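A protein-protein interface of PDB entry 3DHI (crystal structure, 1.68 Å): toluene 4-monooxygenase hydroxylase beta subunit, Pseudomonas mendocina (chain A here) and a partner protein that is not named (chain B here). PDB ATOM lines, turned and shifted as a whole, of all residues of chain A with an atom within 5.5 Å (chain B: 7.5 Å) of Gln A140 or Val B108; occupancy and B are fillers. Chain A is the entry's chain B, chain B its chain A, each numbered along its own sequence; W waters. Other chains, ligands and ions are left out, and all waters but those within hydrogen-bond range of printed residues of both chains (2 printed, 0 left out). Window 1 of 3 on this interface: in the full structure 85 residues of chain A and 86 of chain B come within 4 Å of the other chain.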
ATOM      1  N   HIS A  33       4.297  15.348   9.398  1.00  0.00           N
ATOM      2  CA  HIS A  33       3.480  15.831   8.262  1.00  0.00           C
ATOM      3  C   HIS A  33       2.153  15.094   8.206  1.00  0.00           C
ATOM      4  O   HIS A  33       2.084  14.016   7.610  1.00  0.00           O
ATOM      5  CB  HIS A  33       4.154  15.597   6.908  1.00  0.00           C
ATOM      6  CG  HIS A  33       5.337  16.464   6.626  1.00  0.00           C
ATOM      7  ND1 HIS A  33       5.511  17.716   7.180  1.00  0.00           N
ATOM      8  CD2 HIS A  33       6.367  16.285   5.769  1.00  0.00           C
ATOM      9  CE1 HIS A  33       6.620  18.251   6.703  1.00  0.00           C
ATOM     10  NE2 HIS A  33       7.158  17.401   5.844  1.00  0.00           N
ATOM     11  N   SER A 135      15.784  27.497  -2.849  1.00  0.00           N
ATOM     12  CA  SER A 135      15.567  26.112  -3.313  1.00  0.00           C
ATOM     13  C   SER A 135      15.412  25.122  -2.150  1.00  0.00           C
ATOM     14  O   SER A 135      14.526  24.250  -2.151  1.00  0.00           O
ATOM     15  CB  SER A 135      16.699  25.680  -4.255  1.00  0.00           C
ATOM     16  OG  SER A 135      16.336  24.464  -4.932  1.00  0.00           O
ATOM     17  N   SER A 136      16.251  25.280  -1.126  1.00  0.00           N
ATOM     18  CA  SER A 136      16.194  24.435   0.061  1.00  0.00           C
ATOM     19  C   SER A 136      14.845  24.599   0.740  1.00  0.00           C
ATOM     20  O   SER A 136      14.266  23.632   1.246  1.00  0.00           O
ATOM     21  CB  SER A 136      17.347  24.798   1.001  1.00  0.00           C
ATOM     22  OG  SER A 136      18.615  24.503   0.385  1.00  0.00           O
ATOM     23  N   ALA A 137      14.344  25.833   0.771  1.00  0.00           N
ATOM     24  CA  ALA A 137      12.996  26.058   1.357  1.00  0.00           C
ATOM     25  C   ALA A 137      11.902  25.354   0.569  1.00  0.00           C
ATOM     26  O   ALA A 137      10.895  24.910   1.132  1.00  0.00           O
ATOM     27  CB  ALA A 137      12.687  27.528   1.450  1.00  0.00           C
ATOM     28  N   TYR A 138      12.086  25.280  -0.749  1.00  0.00           N
ATOM     29  CA  TYR A 138      11.087  24.601  -1.564  1.00  0.00           C
ATOM     30  C   TYR A 138      11.084  23.101  -1.258  1.00  0.00           C
ATOM     31  O   TYR A 138      10.019  22.486  -1.049  1.00  0.00           O
ATOM     32  CB  TYR A 138      11.293  24.861  -3.080  1.00  0.00           C
ATOM     33  CG  TYR A 138      10.146  24.229  -3.830  1.00  0.00           C
ATOM     34  CD1 TYR A 138      10.338  23.073  -4.594  1.00  0.00           C
ATOM     35  CD2 TYR A 138       8.846  24.737  -3.705  1.00  0.00           C
ATOM     36  CE1 TYR A 138       9.265  22.457  -5.238  1.00  0.00           C
ATOM     37  CE2 TYR A 138       7.767  24.144  -4.361  1.00  0.00           C
ATOM     38  CZ  TYR A 138       7.982  23.001  -5.110  1.00  0.00           C
ATOM     39  OH  TYR A 138       6.922  22.382  -5.732  1.00  0.00           O
ATOM     40  N   VAL A 139      12.266  22.487  -1.215  1.00  0.00           N
ATOM     41  CA  VAL A 139      12.315  21.070  -0.851  1.00  0.00           C
ATOM     42  C   VAL A 139      11.714  20.844   0.547  1.00  0.00           C
ATOM     43  O   VAL A 139      10.943  19.916   0.740  1.00  0.00           O
ATOM     44  CB  VAL A 139      13.710  20.466  -0.941  1.00  0.00           C
ATOM     45  CG1 VAL A 139      13.617  18.950  -0.770  1.00  0.00           C
ATOM     46  CG2 VAL A 139      14.358  20.821  -2.279  1.00  0.00           C
ATOM     47  N   GLN A 140      12.020  21.729   1.505  1.00  0.00           N
ATOM     48  CA  GLN A 140      11.368  21.681   2.817  1.00  0.00           C
ATOM     49  C   GLN A 140       9.851  21.531   2.732  1.00  0.00           C
ATOM     50  O   GLN A 140       9.282  20.625   3.324  1.00  0.00           O
ATOM     51  CB  GLN A 140      11.712  22.938   3.671  1.00  0.00           C
ATOM     52  CG  GLN A 140      10.943  22.981   5.010  1.00  0.00           C
ATOM     53  CD  GLN A 140       9.588  23.670   4.880  1.00  0.00           C
ATOM     54  OE1 GLN A 140       9.481  24.723   4.243  1.00  0.00           O
ATOM     55  NE2 GLN A 140       8.543  23.052   5.437  1.00  0.00           N
ATOM     56  N   GLN A 141       9.193  22.436   2.014  1.00  0.00           N
ATOM     57  CA  GLN A 141       7.736  22.514   2.076  1.00  0.00           C
ATOM     58  C   GLN A 141       7.044  21.381   1.310  1.00  0.00           C
ATOM     59  O   GLN A 141       5.888  21.105   1.541  1.00  0.00           O
ATOM     60  CB  GLN A 141       7.228  23.911   1.645  1.00  0.00           C
ATOM     61  CG  GLN A 141       7.451  24.254   0.184  1.00  0.00           C
ATOM     62  CD  GLN A 141       7.535  25.741  -0.057  1.00  0.00           C
ATOM     63  OE1 GLN A 141       8.504  26.425   0.348  1.00  0.00           O
ATOM     64  NE2 GLN A 141       6.570  26.254  -0.739  1.00  0.00           N
ATOM     65  N   MET A 142       7.791  20.717   0.434  1.00  0.00           N
ATOM     66  CA  MET A 142       7.237  19.673  -0.432  1.00  0.00           C
ATOM     67  C   MET A 142       7.613  18.237  -0.027  1.00  0.00           C
ATOM     68  O   MET A 142       6.958  17.291  -0.469  1.00  0.00           O
ATOM     69  CB  MET A 142       7.698  19.908  -1.882  1.00  0.00           C
ATOM     70  CG  MET A 142       7.239  21.239  -2.517  1.00  0.00           C
ATOM     71  SD  MET A 142       5.471  21.551  -2.319  1.00  0.00           S
ATOM     72  CE  MET A 142       4.695  20.013  -2.881  1.00  0.00           C
ATOM     73  N   ALA A 143       8.667  18.063   0.770  1.00  0.00           N
ATOM     74  CA  ALA A 143       9.169  16.708   1.082  1.00  0.00           C
ATOM     75  C   ALA A 143       8.120  15.895   1.845  1.00  0.00           C
ATOM     76  O   ALA A 143       7.371  16.452   2.670  1.00  0.00           O
ATOM     77  CB  ALA A 143      10.498  16.779   1.873  1.00  0.00           C
ATOM     78  N   SER A 149      12.153  17.012   5.679  1.00  0.00           N
ATOM     79  CA  SER A 149      11.944  18.463   5.753  1.00  0.00           C
ATOM     80  C   SER A 149      12.898  19.161   6.730  1.00  0.00           C
ATOM     81  O   SER A 149      13.424  20.234   6.398  1.00  0.00           O
ATOM     82  CB  SER A 149      10.469  18.779   6.082  1.00  0.00           C
ATOM     83  OG  SER A 149       9.641  18.427   4.967  1.00  0.00           O
ATOM     84  N   CYS A 152      16.141  19.891   5.303  1.00  0.00           N
ATOM     85  CA  CYS A 152      16.018  21.023   4.395  1.00  0.00           C
ATOM     86  C   CYS A 152      15.933  22.344   5.146  1.00  0.00           C
ATOM     87  O   CYS A 152      16.496  23.336   4.675  1.00  0.00           O
ATOM     88  CB  CYS A 152      14.799  20.888   3.498  1.00  0.00           C
ATOM     89  SG  CYS A 152      14.918  19.384   2.462  1.00  0.00           S
ATOM     90  N   ILE A 153      15.238  22.354   6.284  1.00  0.00           N
ATOM     91  CA  ILE A 153      15.144  23.596   7.091  1.00  0.00           C
ATOM     92  C   ILE A 153      16.565  24.054   7.498  1.00  0.00           C
ATOM     93  O   ILE A 153      16.968  25.203   7.262  1.00  0.00           O
ATOM     94  CB  ILE A 153      14.299  23.441   8.368  1.00  0.00           C
ATOM     95  CG1 ILE A 153      12.824  23.147   8.068  1.00  0.00           C
ATOM     96  CG2 ILE A 153      14.379  24.756   9.216  1.00  0.00           C
ATOM     97  CD1 ILE A 153      12.103  22.592   9.269  1.00  0.00           C
ATOM     98  N   THR A 156      18.480  25.323   4.627  1.00  0.00           N
ATOM     99  CA  THR A 156      18.045  26.662   4.205  1.00  0.00           C
ATOM    100  C   THR A 156      18.767  27.714   5.071  1.00  0.00           C
ATOM    101  O   THR A 156      19.305  28.694   4.559  1.00  0.00           O
ATOM    102  CB  THR A 156      16.517  26.832   4.368  1.00  0.00           C
ATOM    103  OG1 THR A 156      15.810  25.791   3.668  1.00  0.00           O
ATOM    104  CG2 THR A 156      16.069  28.204   3.863  1.00  0.00           C
ATOM    105  N   VAL B 102       1.796  20.297  16.748  1.00  0.00           N
ATOM    106  CA  VAL B 102       2.013  19.879  15.362  1.00  0.00           C
ATOM    107  C   VAL B 102       1.582  20.985  14.395  1.00  0.00           C
ATOM    108  O   VAL B 102       2.086  21.078  13.253  1.00  0.00           O
ATOM    109  CB  VAL B 102       1.384  18.484  15.069  1.00  0.00           C
ATOM    110  CG1 VAL B 102       1.502  18.129  13.567  1.00  0.00           C
ATOM    111  CG2 VAL B 102       2.147  17.428  15.886  1.00  0.00           C
ATOM    112  N   GLY B 103       0.695  21.856  14.871  1.00  0.00           N
ATOM    113  CA  GLY B 103       0.369  23.063  14.116  1.00  0.00           C
ATOM    114  C   GLY B 103       1.554  24.025  14.003  1.00  0.00           C
ATOM    115  O   GLY B 103       1.747  24.659  12.967  1.00  0.00           O
ATOM    116  N   GLU B 104       2.342  24.149  15.068  1.00  0.00           N
ATOM    117  CA  GLU B 104       3.584  24.934  15.027  1.00  0.00           C
ATOM    118  C   GLU B 104       4.482  24.374  13.938  1.00  0.00           C
ATOM    119  O   GLU B 104       5.046  25.111  13.168  1.00  0.00           O
ATOM    120  CB  GLU B 104       4.364  24.860  16.343  1.00  0.00           C
ATOM    121  CG  GLU B 104       3.660  25.501  17.514  1.00  0.00           C
ATOM    122  CD  GLU B 104       3.977  26.973  17.679  1.00  0.00           C
ATOM    123  OE1 GLU B 104       3.765  27.492  18.783  1.00  0.00           O
ATOM    124  OE2 GLU B 104       4.430  27.608  16.705  1.00  0.00           O
ATOM    125  N   TYR B 105       4.589  23.046  13.868  1.00  0.00           N
ATOM    126  CA  TYR B 105       5.446  22.458  12.840  1.00  0.00           C
ATOM    127  C   TYR B 105       4.872  22.731  11.435  1.00  0.00           C
ATOM    128  O   TYR B 105       5.618  22.967  10.492  1.00  0.00           O
ATOM    129  CB  TYR B 105       5.630  20.946  13.093  1.00  0.00           C
ATOM    130  CG  TYR B 105       6.630  20.379  12.134  1.00  0.00           C
ATOM    131  CD1 TYR B 105       7.990  20.599  12.315  1.00  0.00           C
ATOM    132  CD2 TYR B 105       6.197  19.659  11.016  1.00  0.00           C
ATOM    133  CE1 TYR B 105       8.934  20.121  11.393  1.00  0.00           C
ATOM    134  CE2 TYR B 105       7.123  19.170  10.081  1.00  0.00           C
ATOM    135  CZ  TYR B 105       8.480  19.403  10.283  1.00  0.00           C
ATOM    136  OH  TYR B 105       9.381  18.926   9.377  1.00  0.00           O
ATOM    137  N   ALA B 106       3.548  22.722  11.295  1.00  0.00           N
ATOM    138  CA  ALA B 106       2.917  23.157  10.028  1.00  0.00           C
ATOM    139  C   ALA B 106       3.274  24.607   9.660  1.00  0.00           C
ATOM    140  O   ALA B 106       3.493  24.912   8.487  1.00  0.00           O
ATOM    141  CB  ALA B 106       1.404  22.956  10.074  1.00  0.00           C
ATOM    142  N   ALA B 107       3.379  25.493  10.661  1.00  0.00           N
ATOM    143  CA  ALA B 107       3.758  26.890  10.418  1.00  0.00           C
ATOM    144  C   ALA B 107       5.129  27.020   9.756  1.00  0.00           C
ATOM    145  O   ALA B 107       5.374  28.015   9.068  1.00  0.00           O
ATOM    146  CB  ALA B 107       3.701  27.720  11.706  1.00  0.00           C
ATOM    147  N   VAL B 108       6.015  26.033   9.934  1.00  0.00           N
ATOM    148  CA  VAL B 108       7.265  26.006   9.145  1.00  0.00           C
ATOM    149  C   VAL B 108       6.979  26.151   7.657  1.00  0.00           C
ATOM    150  O   VAL B 108       7.681  26.878   6.937  1.00  0.00           O
ATOM    151  CB  VAL B 108       8.081  24.699   9.340  1.00  0.00           C
ATOM    152  CG1 VAL B 108       9.351  24.733   8.436  1.00  0.00           C
ATOM    153  CG2 VAL B 108       8.487  24.524  10.793  1.00  0.00           C
ATOM    154  N   THR B 109       5.929  25.465   7.207  1.00  0.00           N
ATOM    155  CA  THR B 109       5.554  25.460   5.785  1.00  0.00           C
ATOM    156  C   THR B 109       5.027  26.832   5.335  1.00  0.00           C
ATOM    157  O   THR B 109       5.332  27.274   4.241  1.00  0.00           O
ATOM    158  CB  THR B 109       4.579  24.307   5.484  1.00  0.00           C
ATOM    159  OG1 THR B 109       5.277  23.059   5.541  1.00  0.00           O
ATOM    160  CG2 THR B 109       3.921  24.463   4.109  1.00  0.00           C
ATOM    161  N   GLY B 110       4.269  27.524   6.192  1.00  0.00           N
ATOM    162  CA  GLY B 110       3.875  28.893   5.871  1.00  0.00           C
ATOM    163  C   GLY B 110       5.092  29.800   5.701  1.00  0.00           C
ATOM    164  O   GLY B 110       5.171  30.583   4.759  1.00  0.00           O
ATOM    165  N   GLU B 111       6.053  29.666   6.609  1.00  0.00           N
ATOM    166  CA  GLU B 111       7.285  30.459   6.516  1.00  0.00           C
ATOM    167  C   GLU B 111       8.080  30.045   5.275  1.00  0.00           C
ATOM    168  O   GLU B 111       8.603  30.917   4.558  1.00  0.00           O
ATOM    169  CB  GLU B 111       8.123  30.310   7.779  1.00  0.00           C
ATOM    170  CG  GLU B 111       7.420  30.876   9.036  1.00  0.00           C
ATOM    171  CD  GLU B 111       7.338  32.417   9.066  1.00  0.00           C
ATOM    172  OE1 GLU B 111       8.182  33.092   8.455  1.00  0.00           O
ATOM    173  OE2 GLU B 111       6.401  32.962   9.718  1.00  0.00           O
ATOM    174  N   GLY B 112       8.138  28.742   5.003  1.00  0.00           N
ATOM    175  CA  GLY B 112       8.864  28.243   3.808  1.00  0.00           C
ATOM    176  C   GLY B 112       8.248  28.744   2.506  1.00  0.00           C
ATOM    177  O   GLY B 112       8.949  29.019   1.518  1.00  0.00           O
ATOM    178  N   ARG B 113       6.929  28.875   2.510  1.00  0.00           N
ATOM    179  CA  ARG B 113       6.202  29.387   1.347  1.00  0.00           C
ATOM    180  C   ARG B 113       6.681  30.802   1.022  1.00  0.00           C
ATOM    181  O   ARG B 113       6.899  31.139  -0.151  1.00  0.00           O
ATOM    182  CB  ARG B 113       4.694  29.332   1.609  1.00  0.00           C
ATOM    183  CG  ARG B 113       3.831  29.394   0.322  1.00  0.00           C
ATOM    184  CD  ARG B 113       3.734  27.995  -0.330  1.00  0.00           C
ATOM    185  NE  ARG B 113       2.909  27.102   0.492  1.00  0.00           N
ATOM    186  CZ  ARG B 113       3.058  25.777   0.555  1.00  0.00           C
ATOM    187  NH1 ARG B 113       4.016  25.166  -0.133  1.00  0.00           N
ATOM    188  NH2 ARG B 113       2.236  25.051   1.312  1.00  0.00           N
ATOM    189  N   MET B 114       6.900  31.619   2.063  1.00  0.00           N
ATOM    190  CA  MET B 114       7.407  32.971   1.893  1.00  0.00           C
ATOM    191  C   MET B 114       8.885  32.961   1.518  1.00  0.00           C
ATOM    192  O   MET B 114       9.318  33.750   0.669  1.00  0.00           O
ATOM    193  CB  MET B 114       7.188  33.802   3.164  1.00  0.00           C
ATOM    194  CG  MET B 114       5.709  34.002   3.487  1.00  0.00           C
ATOM    195  SD  MET B 114       5.438  35.181   4.839  1.00  0.00           S
ATOM    196  CE  MET B 114       6.071  34.211   6.215  1.00  0.00           C
ATOM    197  N   ALA B 115       9.662  32.075   2.146  1.00  0.00           N
ATOM    198  CA  ALA B 115      11.108  32.021   1.887  1.00  0.00           C
ATOM    199  C   ALA B 115      11.433  31.698   0.418  1.00  0.00           C
ATOM    200  O   ALA B 115      12.400  32.230  -0.123  1.00  0.00           O
ATOM    201  CB  ALA B 115      11.776  31.027   2.788  1.00  0.00           C
ATOM    202  N   ALA B 127      11.745  35.151   6.685  1.00  0.00           N
ATOM    203  CA  ALA B 127      10.972  33.904   6.656  1.00  0.00           C
ATOM    204  C   ALA B 127      11.862  32.668   6.887  1.00  0.00           C
ATOM    205  O   ALA B 127      11.394  31.642   7.377  1.00  0.00           O
ATOM    206  CB  ALA B 127      10.200  33.783   5.363  1.00  0.00           C
ATOM    207  N   GLY B 130      12.016  32.623  10.321  1.00  0.00           N
ATOM    208  CA  GLY B 130      10.666  32.166  10.732  1.00  0.00           C
ATOM    209  C   GLY B 130      10.535  30.644  10.648  1.00  0.00           C
ATOM    210  O   GLY B 130       9.978  30.020  11.525  1.00  0.00           O
ATOM    211  N   MET B 131      11.088  30.042   9.587  1.00  0.00           N
ATOM    212  CA  MET B 131      11.103  28.570   9.456  1.00  0.00           C
ATOM    213  C   MET B 131      11.804  27.950  10.665  1.00  0.00           C
ATOM    214  O   MET B 131      11.336  26.974  11.254  1.00  0.00           O
ATOM    215  CB  MET B 131      11.846  28.141   8.170  1.00  0.00           C
ATOM    216  CG  MET B 131      11.096  28.457   6.871  1.00  0.00           C
ATOM    217  SD  MET B 131      12.243  28.250   5.471  1.00  0.00           S
ATOM    218  CE  MET B 131      12.392  26.467   5.360  1.00  0.00           C
ATOM    219  N   MET B 132      12.959  28.514  11.014  1.00  0.00           N
ATOM    220  CA  MET B 132      13.728  28.027  12.153  1.00  0.00           C
ATOM    221  C   MET B 132      12.950  28.203  13.455  1.00  0.00           C
ATOM    222  O   MET B 132      12.884  27.282  14.278  1.00  0.00           O
ATOM    223  CB  MET B 132      15.070  28.751  12.195  1.00  0.00           C
ATOM    224  CG  MET B 132      15.994  28.277  11.051  1.00  0.00           C
ATOM    225  SD  MET B 132      16.673  26.602  11.385  1.00  0.00           S
ATOM    226  CE  MET B 132      17.818  26.917  12.740  1.00  0.00           C
ATOM    227  N   ASP B 133      12.319  29.358  13.604  1.00  0.00           N
ATOM    228  CA  ASP B 133      11.520  29.635  14.814  1.00  0.00           C
ATOM    229  C   ASP B 133      10.397  28.609  14.993  1.00  0.00           C
ATOM    230  O   ASP B 133      10.166  28.101  16.109  1.00  0.00           O
ATOM    231  CB  ASP B 133      10.859  31.019  14.736  1.00  0.00           C
ATOM    232  CG  ASP B 133      11.856  32.185  14.864  1.00  0.00           C
ATOM    233  OD1 ASP B 133      12.981  32.014  15.350  1.00  0.00           O
ATOM    234  OD2 ASP B 133      11.478  33.301  14.458  1.00  0.00           O
ATOM    235  N   GLU B 134       9.659  28.332  13.925  1.00  0.00           N
ATOM    236  CA  GLU B 134       8.536  27.398  14.057  1.00  0.00           C
ATOM    237  C   GLU B 134       9.026  25.975  14.267  1.00  0.00           C
ATOM    238  O   GLU B 134       8.348  25.208  14.951  1.00  0.00           O
ATOM    239  CB  GLU B 134       7.596  27.444  12.880  1.00  0.00           C
ATOM    240  CG  GLU B 134       7.106  28.835  12.501  1.00  0.00           C
ATOM    241  CD  GLU B 134       6.226  29.498  13.549  1.00  0.00           C
ATOM    242  OE1 GLU B 134       6.168  29.073  14.728  1.00  0.00           O
ATOM    243  OE2 GLU B 134       5.570  30.476  13.172  1.00  0.00           O
ATOM    244  N   LEU B 135      10.149  25.620  13.754  1.00  0.00           N
ATOM    245  CA  LEU B 135      10.773  24.339  14.068  1.00  0.00           C
ATOM    246  C   LEU B 135      11.063  24.217  15.559  1.00  0.00           C
ATOM    247  O   LEU B 135      10.690  23.248  16.228  1.00  0.00           O
ATOM    248  CB  LEU B 135      12.064  24.163  13.265  1.00  0.00           C
ATOM    249  CG  LEU B 135      12.867  22.891  13.546  1.00  0.00           C
ATOM    250  CD1 LEU B 135      12.061  21.656  13.173  1.00  0.00           C
ATOM    251  CD2 LEU B 135      14.193  22.916  12.801  1.00  0.00           C
ATOM    252  N   ARG B 136      11.639  25.314  16.114  1.00  0.00           N
ATOM    253  CA  ARG B 136      11.824  25.375  17.562  1.00  0.00           C
ATOM    254  C   ARG B 136      10.501  25.147  18.282  1.00  0.00           C
ATOM    255  O   ARG B 136      10.435  24.387  19.233  1.00  0.00           O
ATOM    256  CB  ARG B 136      12.363  26.751  17.963  1.00  0.00           C
ATOM    257  CG  ARG B 136      12.563  26.916  19.490  1.00  0.00           C
ATOM    258  CD  ARG B 136      12.893  28.352  19.889  1.00  0.00           C
ATOM    259  NE  ARG B 136      13.226  28.364  21.311  1.00  0.00           N
ATOM    260  CZ  ARG B 136      12.806  29.237  22.225  1.00  0.00           C
ATOM    261  NH1 ARG B 136      12.046  30.289  21.897  1.00  0.00           N
ATOM    262  NH2 ARG B 136      13.174  29.036  23.495  1.00  0.00           N
ATOM    263  N   HIS B 137       9.458  25.841  17.845  1.00  0.00           N
ATOM    264  CA  HIS B 137       8.202  25.812  18.612  1.00  0.00           C
ATOM    265  C   HIS B 137       7.560  24.443  18.555  1.00  0.00           C
ATOM    266  O   HIS B 137       7.026  23.994  19.563  1.00  0.00           O
ATOM    267  CB  HIS B 137       7.244  26.874  18.099  1.00  0.00           C
ATOM    268  CG  HIS B 137       7.803  28.264  18.204  1.00  0.00           C
ATOM    269  ND1 HIS B 137       7.219  29.348  17.596  1.00  0.00           N
ATOM    270  CD2 HIS B 137       8.915  28.732  18.831  1.00  0.00           C
ATOM    271  CE1 HIS B 137       7.944  30.433  17.848  1.00  0.00           C
ATOM    272  NE2 HIS B 137       8.979  30.084  18.595  1.00  0.00           N
ATOM    273  N   GLY B 138       7.624  23.787  17.392  1.00  0.00           N
ATOM    274  CA  GLY B 138       7.094  22.419  17.259  1.00  0.00           C
ATOM    275  C   GLY B 138       7.869  21.447  18.135  1.00  0.00           C
ATOM    276  O   GLY B 138       7.276  20.600  18.833  1.00  0.00           O
ATOM    277  N   ILE B 180      -2.340  29.126   6.744  1.00  0.00           N
ATOM    278  CA  ILE B 180      -0.897  28.922   6.838  1.00  0.00           C
ATOM    279  C   ILE B 180      -0.326  28.134   5.672  1.00  0.00           C
ATOM    280  O   ILE B 180       0.608  28.589   5.025  1.00  0.00           O
ATOM    281  CB  ILE B 180      -0.466  28.245   8.180  1.00  0.00           C
ATOM    282  CG1 ILE B 180      -0.885  29.088   9.383  1.00  0.00           C
ATOM    283  CG2 ILE B 180       1.039  28.014   8.216  1.00  0.00           C
ATOM    284  CD1 ILE B 180      -0.321  28.549  10.705  1.00  0.00           C
ATOM    285  N   THR B 181      -0.871  26.948   5.424  1.00  0.00           N
ATOM    286  CA  THR B 181      -0.247  26.032   4.465  1.00  0.00           C
ATOM    287  C   THR B 181      -0.959  25.993   3.124  1.00  0.00           C
ATOM    288  O   THR B 181      -0.408  25.465   2.148  1.00  0.00           O
ATOM    289  CB  THR B 181      -0.177  24.608   4.993  1.00  0.00           C
ATOM    290  OG1 THR B 181      -1.516  24.135   5.216  1.00  0.00           O
ATOM    291  CG2 THR B 181       0.643  24.556   6.310  1.00  0.00           C
ATOM    292  N   LEU B 192      -1.261  35.079   8.335  1.00  0.00           N
ATOM    293  CA  LEU B 192      -0.630  34.371   9.432  1.00  0.00           C
ATOM    294  C   LEU B 192       0.111  35.381  10.292  1.00  0.00           C
ATOM    295  O   LEU B 192      -0.192  35.518  11.469  1.00  0.00           O
ATOM    296  CB  LEU B 192       0.340  33.276   8.946  1.00  0.00           C
ATOM    297  CG  LEU B 192       1.330  32.681   9.962  1.00  0.00           C
ATOM    298  CD1 LEU B 192       0.592  32.075  11.139  1.00  0.00           C
ATOM    299  CD2 LEU B 192       2.141  31.611   9.243  1.00  0.00           C
HETATM  300  O   HOH W   1       8.411  21.015   7.519  1.00  0.00           O
HETATM  301  O   HOH W   2       4.439  21.206   3.830  1.00  0.00           O
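Water W2 lies within hydrogen-bond range of the side-chain hydroxyl of Thr B109 (2.7 Å) and the backbone carbonyl oxygen of Gln A141 (2.7 Å). Water W1 bridges NE2 of Gln A140 and OH of Tyr B105.
Of the 14 printed residues of chain A, 7 touch a printed residue of chain B. Printed residues of chain A that touch a printed residue of chain B: His A33, Ala A137, Gln A140, Gln A141, Ser A149, Ile A153 and Thr A156. Hydrophobic or aromatic side chains of chain A that line the printed part of chain B: His A33, Ala A137 and Ile A153. Of the 27 printed residues of chain B, 8 touch a printed residue of chain A. Printed residues of chain B that touch a printed residue of chain A: Tyr B105, Val B108, Thr B109, Gly B112, Arg B113, Ala B115, Met B131 and Met B132. Among the printed residues, 12 pairs touch across the chains. Among the printed residues, no Asp or Glu carboxylate lies within 4 Å of a Lys or Arg side-chain nitrogen of the other chain.
Tyr B105 touches His A33. CB of Ala A137 touches CB of Ala B115, 3.9 Å away. Gln A140 touches Val B108 (NE2 to CG1, 3.5 Å). Gln A140 touches Gly B112 (OE1 to CA, 3.6 Å). Met B131 touches Gln A140 (CE to OE1, 3.6 Å). Tyr B105 touches Ser A149. CD1 of Ile A153 touches CG1 of Val B108, at 3.6 Å. Ile A153 touches Met B132 (CG2 to SD, 3.7 Å). OG1 of Thr A156 touches CE of Met B131, 3.9 Å away.
The side-chain amide nitrogen (NE2) of Gln A140 is in hydrogen-bond range of the side-chain hydroxyl (OG1) of Thr B109 (3.3 Å). The backbone carbonyl oxygen of Gly B112 sits close to the side-chain amide oxygen of Gln A141 (2.9 Å). NH1 of Arg B113 sits close to NE2 of Gln A141 (2.8 Å).
NH2 of Arg B113 is in hydrogen-bond range of O of Thr B181 (2.8 Å). A ring nitrogen (NE2) of His A33 lies close to the backbone carbonyl oxygen of Ala A143. OE1 of Gln A140 sits close to O of Ala A137 (3.4 Å). The side-chain amide oxygen (OE1) of Gln A141 sits close to the backbone carbonyl oxygen (O) of Ala A137, at 2.9 Å. The backbone carbonyl oxygen (O) of Gln A140 is in hydrogen-bond range of the side-chain hydroxyl (OG) of Ser A149, 2.8 Å away. The backbone carbonyl oxygen of Cys A152 is in hydrogen-bond range of the side-chain hydroxyl of Thr A156 (2.7 Å).
Of the printed residues of chain B, Ala A137 touches Ala B115 (3.9 Å). Of the printed residues of chain A, Tyr B105 touches His A33 (3.5 Å) and Ser A149 (3.5 Å). Val B108 touches two residues of chain A. Of the printed residues of chain A, Gly B112 touches Gln A140 and Gln A141.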
